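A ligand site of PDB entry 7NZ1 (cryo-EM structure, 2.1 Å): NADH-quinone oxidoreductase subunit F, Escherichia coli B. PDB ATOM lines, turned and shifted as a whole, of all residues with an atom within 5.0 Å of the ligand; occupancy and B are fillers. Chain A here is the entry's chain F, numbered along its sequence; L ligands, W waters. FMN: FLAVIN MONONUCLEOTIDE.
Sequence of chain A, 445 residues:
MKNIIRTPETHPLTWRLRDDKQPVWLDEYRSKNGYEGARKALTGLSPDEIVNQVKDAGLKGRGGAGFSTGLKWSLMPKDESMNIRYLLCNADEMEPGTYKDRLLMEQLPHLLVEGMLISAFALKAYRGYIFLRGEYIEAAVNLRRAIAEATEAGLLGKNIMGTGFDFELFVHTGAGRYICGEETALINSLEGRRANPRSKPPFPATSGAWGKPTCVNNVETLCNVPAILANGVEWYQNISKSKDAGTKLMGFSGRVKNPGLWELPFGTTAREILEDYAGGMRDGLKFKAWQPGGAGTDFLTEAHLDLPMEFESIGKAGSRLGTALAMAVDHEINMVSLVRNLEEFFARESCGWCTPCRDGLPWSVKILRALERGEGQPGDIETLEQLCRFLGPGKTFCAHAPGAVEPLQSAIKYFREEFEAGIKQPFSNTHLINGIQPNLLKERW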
ATOM      1  N   GLY A  61      -2.607 -16.648  16.342  1.00  0.00           N
ATOM      2  CA  GLY A  61      -4.036 -16.879  16.475  1.00  0.00           C
ATOM      3  C   GLY A  61      -4.854 -16.033  15.526  1.00  0.00           C
ATOM      4  O   GLY A  61      -4.591 -14.838  15.340  1.00  0.00           O
ATOM      5  N   ARG A  62      -5.854 -16.658  14.912  1.00  0.00           N
ATOM      6  CA  ARG A  62      -6.686 -16.027  13.908  1.00  0.00           C
ATOM      7  C   ARG A  62      -7.984 -15.465  14.482  1.00  0.00           C
ATOM      8  O   ARG A  62      -8.848 -15.027  13.718  1.00  0.00           O
ATOM      9  CB  ARG A  62      -7.012 -17.017  12.785  1.00  0.00           C
ATOM     10  CG  ARG A  62      -5.813 -17.849  12.312  1.00  0.00           C
ATOM     11  CD  ARG A  62      -4.734 -16.973  11.694  1.00  0.00           C
ATOM     12  NE  ARG A  62      -3.915 -17.697  10.726  1.00  0.00           N
ATOM     13  CZ  ARG A  62      -2.592 -17.742  10.745  1.00  0.00           C
ATOM     14  NH1 ARG A  62      -1.888 -17.113  11.679  1.00  0.00           N
ATOM     15  NH2 ARG A  62      -1.944 -18.443   9.815  1.00  0.00           N
ATOM     16  N   GLY A  63      -8.139 -15.472  15.807  1.00  0.00           N
ATOM     17  CA  GLY A  63      -9.356 -14.983  16.433  1.00  0.00           C
ATOM     18  C   GLY A  63      -9.495 -13.488  16.500  1.00  0.00           C
ATOM     19  O   GLY A  63     -10.589 -12.992  16.801  1.00  0.00           O
ATOM     20  N   GLY A  64      -8.423 -12.734  16.231  1.00  0.00           N
ATOM     21  CA  GLY A  64      -8.464 -11.289  16.269  1.00  0.00           C
ATOM     22  C   GLY A  64      -7.455 -10.643  17.200  1.00  0.00           C
ATOM     23  O   GLY A  64      -7.452  -9.409  17.299  1.00  0.00           O
ATOM     24  N   ALA A  65      -6.601 -11.399  17.890  1.00  0.00           N
ATOM     25  CA  ALA A  65      -5.560 -10.826  18.727  1.00  0.00           C
ATOM     26  C   ALA A  65      -4.154 -11.145  18.234  1.00  0.00           C
ATOM     27  O   ALA A  65      -3.268 -10.288  18.364  1.00  0.00           O
ATOM     28  CB  ALA A  65      -5.706 -11.299  20.176  1.00  0.00           C
ATOM     29  N   PHE A  67      -1.893 -13.599  19.197  1.00  0.00           N
ATOM     30  CA  PHE A  67      -0.886 -14.156  20.095  1.00  0.00           C
ATOM     31  C   PHE A  67      -0.302 -15.429  19.489  1.00  0.00           C
ATOM     32  O   PHE A  67      -0.929 -16.093  18.675  1.00  0.00           O
ATOM     33  CB  PHE A  67      -1.503 -14.446  21.465  1.00  0.00           C
ATOM     34  CG  PHE A  67      -0.485 -14.660  22.562  1.00  0.00           C
ATOM     35  CD1 PHE A  67       0.244 -13.595  23.089  1.00  0.00           C
ATOM     36  CD2 PHE A  67      -0.272 -15.925  23.081  1.00  0.00           C
ATOM     37  CE1 PHE A  67       1.156 -13.790  24.094  1.00  0.00           C
ATOM     38  CE2 PHE A  67       0.649 -16.140  24.094  1.00  0.00           C
ATOM     39  CZ  PHE A  67       1.370 -15.063  24.602  1.00  0.00           C
ATOM     40  N   LYS A  72       1.502 -19.904  23.805  1.00  0.00           N
ATOM     41  CA  LYS A  72       0.307 -20.159  24.615  1.00  0.00           C
ATOM     42  C   LYS A  72       0.211 -21.621  25.026  1.00  0.00           C
ATOM     43  O   LYS A  72      -0.133 -21.935  26.172  1.00  0.00           O
ATOM     44  CB  LYS A  72      -0.939 -19.711  23.839  1.00  0.00           C
ATOM     45  CG  LYS A  72      -2.245 -20.279  24.332  1.00  0.00           C
ATOM     46  CD  LYS A  72      -3.366 -20.166  23.302  1.00  0.00           C
ATOM     47  CE  LYS A  72      -4.054 -18.821  23.361  1.00  0.00           C
ATOM     48  NZ  LYS A  72      -5.142 -18.694  22.358  1.00  0.00           N
ATOM     49  N   ASN A  90     -12.906 -22.350  19.539  1.00  0.00           N
ATOM     50  CA  ASN A  90     -13.770 -21.170  19.469  1.00  0.00           C
ATOM     51  C   ASN A  90     -14.403 -21.108  18.083  1.00  0.00           C
ATOM     52  O   ASN A  90     -13.806 -20.600  17.135  1.00  0.00           O
ATOM     53  CB  ASN A  90     -12.972 -19.911  19.792  1.00  0.00           C
ATOM     54  CG  ASN A  90     -13.854 -18.740  20.207  1.00  0.00           C
ATOM     55  OD1 ASN A  90     -15.001 -18.632  19.793  1.00  0.00           O
ATOM     56  ND2 ASN A  90     -13.314 -17.865  21.031  1.00  0.00           N
ATOM     57  N   ASP A  92     -17.366 -19.493  17.623  1.00  0.00           N
ATOM     58  CA  ASP A  92     -18.468 -18.589  17.908  1.00  0.00           C
ATOM     59  C   ASP A  92     -18.807 -17.740  16.685  1.00  0.00           C
ATOM     60  O   ASP A  92     -19.903 -17.856  16.144  1.00  0.00           O
ATOM     61  CB  ASP A  92     -18.148 -17.735  19.137  1.00  0.00           C
ATOM     62  CG  ASP A  92     -19.404 -17.236  19.854  1.00  0.00           C
ATOM     63  OD1 ASP A  92     -20.339 -18.041  20.060  1.00  0.00           O
ATOM     64  OD2 ASP A  92     -19.436 -16.052  20.242  1.00  0.00           O
ATOM     65  N   GLU A  93     -17.826 -16.965  16.189  1.00  0.00           N
ATOM     66  CA  GLU A  93     -17.934 -16.108  14.994  1.00  0.00           C
ATOM     67  C   GLU A  93     -19.176 -15.205  15.059  1.00  0.00           C
ATOM     68  O   GLU A  93     -20.171 -15.378  14.349  1.00  0.00           O
ATOM     69  CB  GLU A  93     -17.886 -16.959  13.704  1.00  0.00           C
ATOM     70  CG  GLU A  93     -17.899 -16.213  12.348  1.00  0.00           C
ATOM     71  CD  GLU A  93     -16.938 -16.724  11.316  1.00  0.00           C
ATOM     72  OE1 GLU A  93     -15.720 -16.537  11.481  1.00  0.00           O
ATOM     73  OE2 GLU A  93     -17.406 -17.361  10.351  1.00  0.00           O
ATOM     74  N   MET A  94     -19.170 -14.309  16.037  1.00  0.00           N
ATOM     75  CA  MET A  94     -20.284 -13.373  16.187  1.00  0.00           C
ATOM     76  C   MET A  94     -19.929 -11.945  15.838  1.00  0.00           C
ATOM     77  O   MET A  94     -20.817 -11.075  15.887  1.00  0.00           O
ATOM     78  CB  MET A  94     -20.840 -13.454  17.610  1.00  0.00           C
ATOM     79  CG  MET A  94     -21.482 -14.773  17.954  1.00  0.00           C
ATOM     80  SD  MET A  94     -23.215 -14.794  17.459  1.00  0.00           S
ATOM     81  CE  MET A  94     -23.907 -13.741  18.722  1.00  0.00           C
ATOM     82  N   GLU A  95     -18.685 -11.654  15.472  1.00  0.00           N
ATOM     83  CA  GLU A  95     -18.329 -10.293  15.103  1.00  0.00           C
ATOM     84  C   GLU A  95     -18.886  -9.973  13.723  1.00  0.00           C
ATOM     85  O   GLU A  95     -18.804 -10.824  12.829  1.00  0.00           O
ATOM     86  CB  GLU A  95     -16.817 -10.097  15.145  1.00  0.00           C
ATOM     87  CG  GLU A  95     -16.371  -8.692  14.746  1.00  0.00           C
ATOM     88  CD  GLU A  95     -15.098  -8.252  15.425  1.00  0.00           C
ATOM     89  OE1 GLU A  95     -15.167  -7.824  16.598  1.00  0.00           O
ATOM     90  OE2 GLU A  95     -14.026  -8.304  14.791  1.00  0.00           O
ATOM     91  N   TYR A 178     -22.628 -12.466  21.806  1.00  0.00           N
ATOM     92  CA  TYR A 178     -21.350 -12.172  21.177  1.00  0.00           C
ATOM     93  C   TYR A 178     -20.191 -12.309  22.164  1.00  0.00           C
ATOM     94  O   TYR A 178     -19.090 -12.711  21.771  1.00  0.00           O
ATOM     95  CB  TYR A 178     -21.375 -10.763  20.551  1.00  0.00           C
ATOM     96  CG  TYR A 178     -20.018 -10.167  20.199  1.00  0.00           C
ATOM     97  CD1 TYR A 178     -19.185 -10.766  19.260  1.00  0.00           C
ATOM     98  CD2 TYR A 178     -19.574  -8.995  20.812  1.00  0.00           C
ATOM     99  CE1 TYR A 178     -17.959 -10.230  18.942  1.00  0.00           C
ATOM    100  CE2 TYR A 178     -18.353  -8.451  20.497  1.00  0.00           C
ATOM    101  CZ  TYR A 178     -17.546  -9.068  19.562  1.00  0.00           C
ATOM    102  OH  TYR A 178     -16.325  -8.533  19.236  1.00  0.00           O
ATOM    103  N   ILE A 179     -20.434 -12.054  23.450  1.00  0.00           N
ATOM    104  CA  ILE A 179     -19.383 -12.134  24.460  1.00  0.00           C
ATOM    105  C   ILE A 179     -18.944 -13.562  24.747  1.00  0.00           C
ATOM    106  O   ILE A 179     -17.863 -13.780  25.299  1.00  0.00           O
ATOM    107  CB  ILE A 179     -19.880 -11.415  25.741  1.00  0.00           C
ATOM    108  CG1 ILE A 179     -18.740 -11.064  26.711  1.00  0.00           C
ATOM    109  CG2 ILE A 179     -20.930 -12.238  26.453  1.00  0.00           C
ATOM    110  CD1 ILE A 179     -17.604 -10.305  26.070  1.00  0.00           C
ATOM    111  N   GLY A 181     -17.679 -15.382  22.533  1.00  0.00           N
ATOM    112  CA  GLY A 181     -16.434 -15.565  21.810  1.00  0.00           C
ATOM    113  C   GLY A 181     -15.196 -15.161  22.570  1.00  0.00           C
ATOM    114  O   GLY A 181     -14.096 -15.600  22.216  1.00  0.00           O
ATOM    115  N   GLU A 182     -15.342 -14.301  23.581  1.00  0.00           N
ATOM    116  CA  GLU A 182     -14.254 -14.009  24.506  1.00  0.00           C
ATOM    117  C   GLU A 182     -13.898 -15.276  25.266  1.00  0.00           C
ATOM    118  O   GLU A 182     -14.774 -15.991  25.755  1.00  0.00           O
ATOM    119  CB  GLU A 182     -14.669 -12.891  25.465  1.00  0.00           C
ATOM    120  CG  GLU A 182     -13.517 -12.122  26.097  1.00  0.00           C
ATOM    121  CD  GLU A 182     -12.939 -12.798  27.308  1.00  0.00           C
ATOM    122  OE1 GLU A 182     -13.635 -13.620  27.934  1.00  0.00           O
ATOM    123  OE2 GLU A 182     -11.777 -12.492  27.658  1.00  0.00           O
ATOM    124  N   GLU A 183     -12.592 -15.553  25.359  1.00  0.00           N
ATOM    125  CA  GLU A 183     -12.121 -16.900  25.691  1.00  0.00           C
ATOM    126  C   GLU A 183     -12.393 -17.271  27.146  1.00  0.00           C
ATOM    127  O   GLU A 183     -12.704 -18.418  27.437  1.00  0.00           O
ATOM    128  CB  GLU A 183     -10.625 -17.038  25.375  1.00  0.00           C
ATOM    129  CG  GLU A 183      -9.741 -15.956  25.939  1.00  0.00           C
ATOM    130  CD  GLU A 183      -8.311 -16.435  26.115  1.00  0.00           C
ATOM    131  OE1 GLU A 183      -8.022 -17.578  25.702  1.00  0.00           O
ATOM    132  OE2 GLU A 183      -7.479 -15.679  26.664  1.00  0.00           O
ATOM    133  N   VAL A 216      -7.870 -22.459  24.632  1.00  0.00           N
ATOM    134  CA  VAL A 216      -8.907 -22.012  23.701  1.00  0.00           C
ATOM    135  C   VAL A 216      -8.295 -21.488  22.408  1.00  0.00           C
ATOM    136  O   VAL A 216      -7.469 -20.590  22.430  1.00  0.00           O
ATOM    137  CB  VAL A 216      -9.803 -20.939  24.328  1.00  0.00           C
ATOM    138  CG1 VAL A 216     -10.956 -20.607  23.404  1.00  0.00           C
ATOM    139  CG2 VAL A 216     -10.315 -21.387  25.673  1.00  0.00           C
ATOM    140  N   ASN A 217      -8.687 -22.071  21.268  1.00  0.00           N
ATOM    141  CA  ASN A 217      -8.142 -21.714  19.969  1.00  0.00           C
ATOM    142  C   ASN A 217      -9.252 -21.553  18.929  1.00  0.00           C
ATOM    143  O   ASN A 217     -10.236 -22.286  18.950  1.00  0.00           O
ATOM    144  CB  ASN A 217      -7.132 -22.738  19.469  1.00  0.00           C
ATOM    145  CG  ASN A 217      -5.835 -22.682  20.246  1.00  0.00           C
ATOM    146  OD1 ASN A 217      -5.667 -23.380  21.244  1.00  0.00           O
ATOM    147  ND2 ASN A 217      -4.928 -21.836  19.798  1.00  0.00           N
ATOM    148  N   ASN A 218      -9.079 -20.567  18.048  1.00  0.00           N
ATOM    149  CA  ASN A 218      -9.973 -20.304  16.935  1.00  0.00           C
ATOM    150  C   ASN A 218      -9.938 -21.473  15.931  1.00  0.00           C
ATOM    151  O   ASN A 218      -8.985 -22.254  15.896  1.00  0.00           O
ATOM    152  CB  ASN A 218      -9.576 -18.965  16.280  1.00  0.00           C
ATOM    153  CG  ASN A 218     -10.457 -18.561  15.101  1.00  0.00           C
ATOM    154  OD1 ASN A 218     -10.059 -18.692  13.947  1.00  0.00           O
ATOM    155  ND2 ASN A 218     -11.656 -18.070  15.392  1.00  0.00           N
ATOM    156  N   THR A 221      -7.114 -21.172  13.340  1.00  0.00           N
ATOM    157  CA  THR A 221      -5.829 -21.518  13.947  1.00  0.00           C
ATOM    158  C   THR A 221      -5.613 -23.025  13.963  1.00  0.00           C
ATOM    159  O   THR A 221      -4.517 -23.507  13.661  1.00  0.00           O
ATOM    160  CB  THR A 221      -5.737 -20.958  15.364  1.00  0.00           C
ATOM    161  OG1 THR A 221      -6.167 -19.590  15.377  1.00  0.00           O
ATOM    162  CG2 THR A 221      -4.314 -21.052  15.884  1.00  0.00           C
ATOM    163  N   ALA A 399     -11.965  -6.948  26.861  1.00  0.00           N
ATOM    164  CA  ALA A 399     -11.610  -6.190  25.662  1.00  0.00           C
ATOM    165  C   ALA A 399     -12.792  -5.806  24.785  1.00  0.00           C
ATOM    166  O   ALA A 399     -12.573  -5.247  23.703  1.00  0.00           O
ATOM    167  CB  ALA A 399     -10.595  -6.974  24.829  1.00  0.00           C
ATOM    168  N   HIS A 400     -14.026  -6.127  25.195  1.00  0.00           N
ATOM    169  CA  HIS A 400     -15.217  -5.769  24.429  1.00  0.00           C
ATOM    170  C   HIS A 400     -15.351  -4.258  24.250  1.00  0.00           C
ATOM    171  O   HIS A 400     -15.524  -3.772  23.121  1.00  0.00           O
ATOM    172  CB  HIS A 400     -16.450  -6.324  25.122  1.00  0.00           C
ATOM    173  CG  HIS A 400     -17.725  -5.960  24.438  1.00  0.00           C
ATOM    174  ND1 HIS A 400     -18.635  -5.102  25.009  1.00  0.00           N
ATOM    175  CD2 HIS A 400     -18.227  -6.298  23.227  1.00  0.00           C
ATOM    176  CE1 HIS A 400     -19.651  -4.944  24.182  1.00  0.00           C
ATOM    177  NE2 HIS A 400     -19.431  -5.657  23.094  1.00  0.00           N
HETATM  178  N1  FMN L   1     -12.234 -15.407  18.983  1.00  0.00           N
HETATM  179  C2  FMN L   1     -12.789 -16.283  18.088  1.00  0.00           C
HETATM  180  O2  FMN L   1     -12.097 -17.177  17.610  1.00  0.00           O
HETATM  181  N3  FMN L   1     -14.104 -16.165  17.723  1.00  0.00           N
HETATM  182  C4  FMN L   1     -14.887 -15.166  18.268  1.00  0.00           C
HETATM  183  O4  FMN L   1     -16.056 -15.073  17.938  1.00  0.00           O
HETATM  184  C4A FMN L   1     -14.327 -14.280  19.184  1.00  0.00           C
HETATM  185  N5  FMN L   1     -15.086 -13.268  19.737  1.00  0.00           N
HETATM  186  C5A FMN L   1     -14.526 -12.391  20.642  1.00  0.00           C
HETATM  187  C6  FMN L   1     -15.314 -11.384  21.189  1.00  0.00           C
HETATM  188  C7  FMN L   1     -14.764 -10.491  22.098  1.00  0.00           C
HETATM  189  C7M FMN L   1     -15.632  -9.421  22.675  1.00  0.00           C
HETATM  190  C8  FMN L   1     -13.427 -10.619  22.462  1.00  0.00           C
HETATM  191  C8M FMN L   1     -12.803  -9.660  23.439  1.00  0.00           C
HETATM  192  C9  FMN L   1     -12.649 -11.618  21.908  1.00  0.00           C
HETATM  193  C9A FMN L   1     -13.189 -12.519  21.005  1.00  0.00           C
HETATM  194  N10 FMN L   1     -12.422 -13.525  20.447  1.00  0.00           N
HETATM  195  C10 FMN L   1     -12.993 -14.395  19.537  1.00  0.00           C
HETATM  196  C1' FMN L   1     -10.963 -13.709  20.814  1.00  0.00           C
HETATM  197  C2' FMN L   1     -10.816 -14.713  21.964  1.00  0.00           C
HETATM  198  O2' FMN L   1     -11.033 -14.094  23.207  1.00  0.00           O
HETATM  199  C3' FMN L   1      -9.441 -15.362  21.965  1.00  0.00           C
HETATM  200  O3' FMN L   1      -8.442 -14.377  21.916  1.00  0.00           O
HETATM  201  C4' FMN L   1      -9.256 -16.338  20.814  1.00  0.00           C
HETATM  202  O4' FMN L   1     -10.306 -17.280  20.773  1.00  0.00           O
HETATM  203  C5' FMN L   1      -7.926 -17.031  20.983  1.00  0.00           C
HETATM  204  O5' FMN L   1      -7.770 -18.067  20.050  1.00  0.00           O
HETATM  205  P   FMN L   1      -6.650 -17.944  18.901  1.00  0.00           P
HETATM  206  O1P FMN L   1      -5.290 -17.942  19.542  1.00  0.00           O
HETATM  207  O2P FMN L   1      -6.738 -19.137  17.992  1.00  0.00           O
HETATM  208  O3P FMN L   1      -6.887 -16.677  18.118  1.00  0.00           O
HETATM  209  O   HOH W   1      -6.716 -14.369  19.366  1.00  0.00           O
HETATM  210  O   HOH W   2     -14.224 -10.334  18.009  1.00  0.00           O
HETATM  211  O   HOH W   3     -15.619 -13.350  15.277  1.00  0.00           O
HETATM  212  O   HOH W   4      -9.811 -11.281  23.570  1.00  0.00           O
HETATM  213  O   HOH W   5     -18.032 -14.090  19.319  1.00  0.00           O
HETATM  214  O   HOH W   6      -2.856 -18.684  19.266  1.00  0.00           O
HETATM  215  O   HOH W   7     -15.243 -18.294  16.301  1.00  0.00           O
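N of Asn 218 sits close to O2P of the ligand (2.7 Å).
The backbone carbonyl oxygen (O) of Val 216 sits close to an oxygen (O5') of the ligand (3.5 Å).
O2 of the ligand sits close to ND2 of Asn 218, 2.4 Å away.
O3P of the ligand sits close to N of Arg 62 (3.4 Å).
The backbone NH (N) of Glu 183 lies close to an oxygen (O2') of the ligand, at 3.0 Å.
OG1 of Thr 221 sits close to O2P of the ligand, 2.7 Å away.
N10 of the ligand lies close to O of Gly 181 (3.2 Å).
The side-chain amino group (NZ) of Lys 72 lies close to an oxygen (O1P) of the ligand, at 2.9 Å.
O3P of the ligand lies close to N of Gly 63 (2.9 Å).
N of Glu 93 lies close to O4 of the ligand, 3.1 Å away.
The side-chain amide nitrogen of Asn 90 sits close to an oxygen (O4') of the ligand, 3.1 Å away.
The side-chain hydroxyl (OG1) of Thr 221 is in hydrogen-bond range of the backbone NH (N) of Arg 62 (3.0 Å).
The backbone carbonyl oxygen (O) of Phe 67 lies within hydrogen-bond range of the backbone NH (N) of Gly 61, 2.9 Å away.
The side-chain amino group (NZ) of Lys 72 is in hydrogen-bond range of the backbone carbonyl oxygen (O) of Val 216.
O of Gly 181 is in hydrogen-bond range of ND2 of Asn 90 (2.7 Å).
The backbone NH of Asp 92 sits at hydrogen-bond distance from the side-chain amide oxygen of Asn 90.
OD2 of Asp 92 lies within hydrogen-bond range of N of Gly 181 (3.0 Å).
N of Asn 90 lies within hydrogen-bond range of O of Asn 217.
The side-chain hydroxyl (OH) of Tyr 178 is in hydrogen-bond range of the side-chain carboxylate (OE1) of Glu 95, 3.0 Å away.
Residues that only touch the ligand: Gly 61, Asp 92, Met 94, Tyr 178, Glu 182, Asn 217 and Ala 399.
Water W5 lies within hydrogen-bond range of the side-chain carboxylate (OD2) of Asp 92, the backbone carbonyl oxygen (O) of Tyr 178, the backbone NH (N) of Met 94 and the backbone NH (N) of Gly 181.
Water W2 lies within hydrogen-bond range of OH of Tyr 178 (3.0 Å) and OE1 of Glu 95 (3.0 Å).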
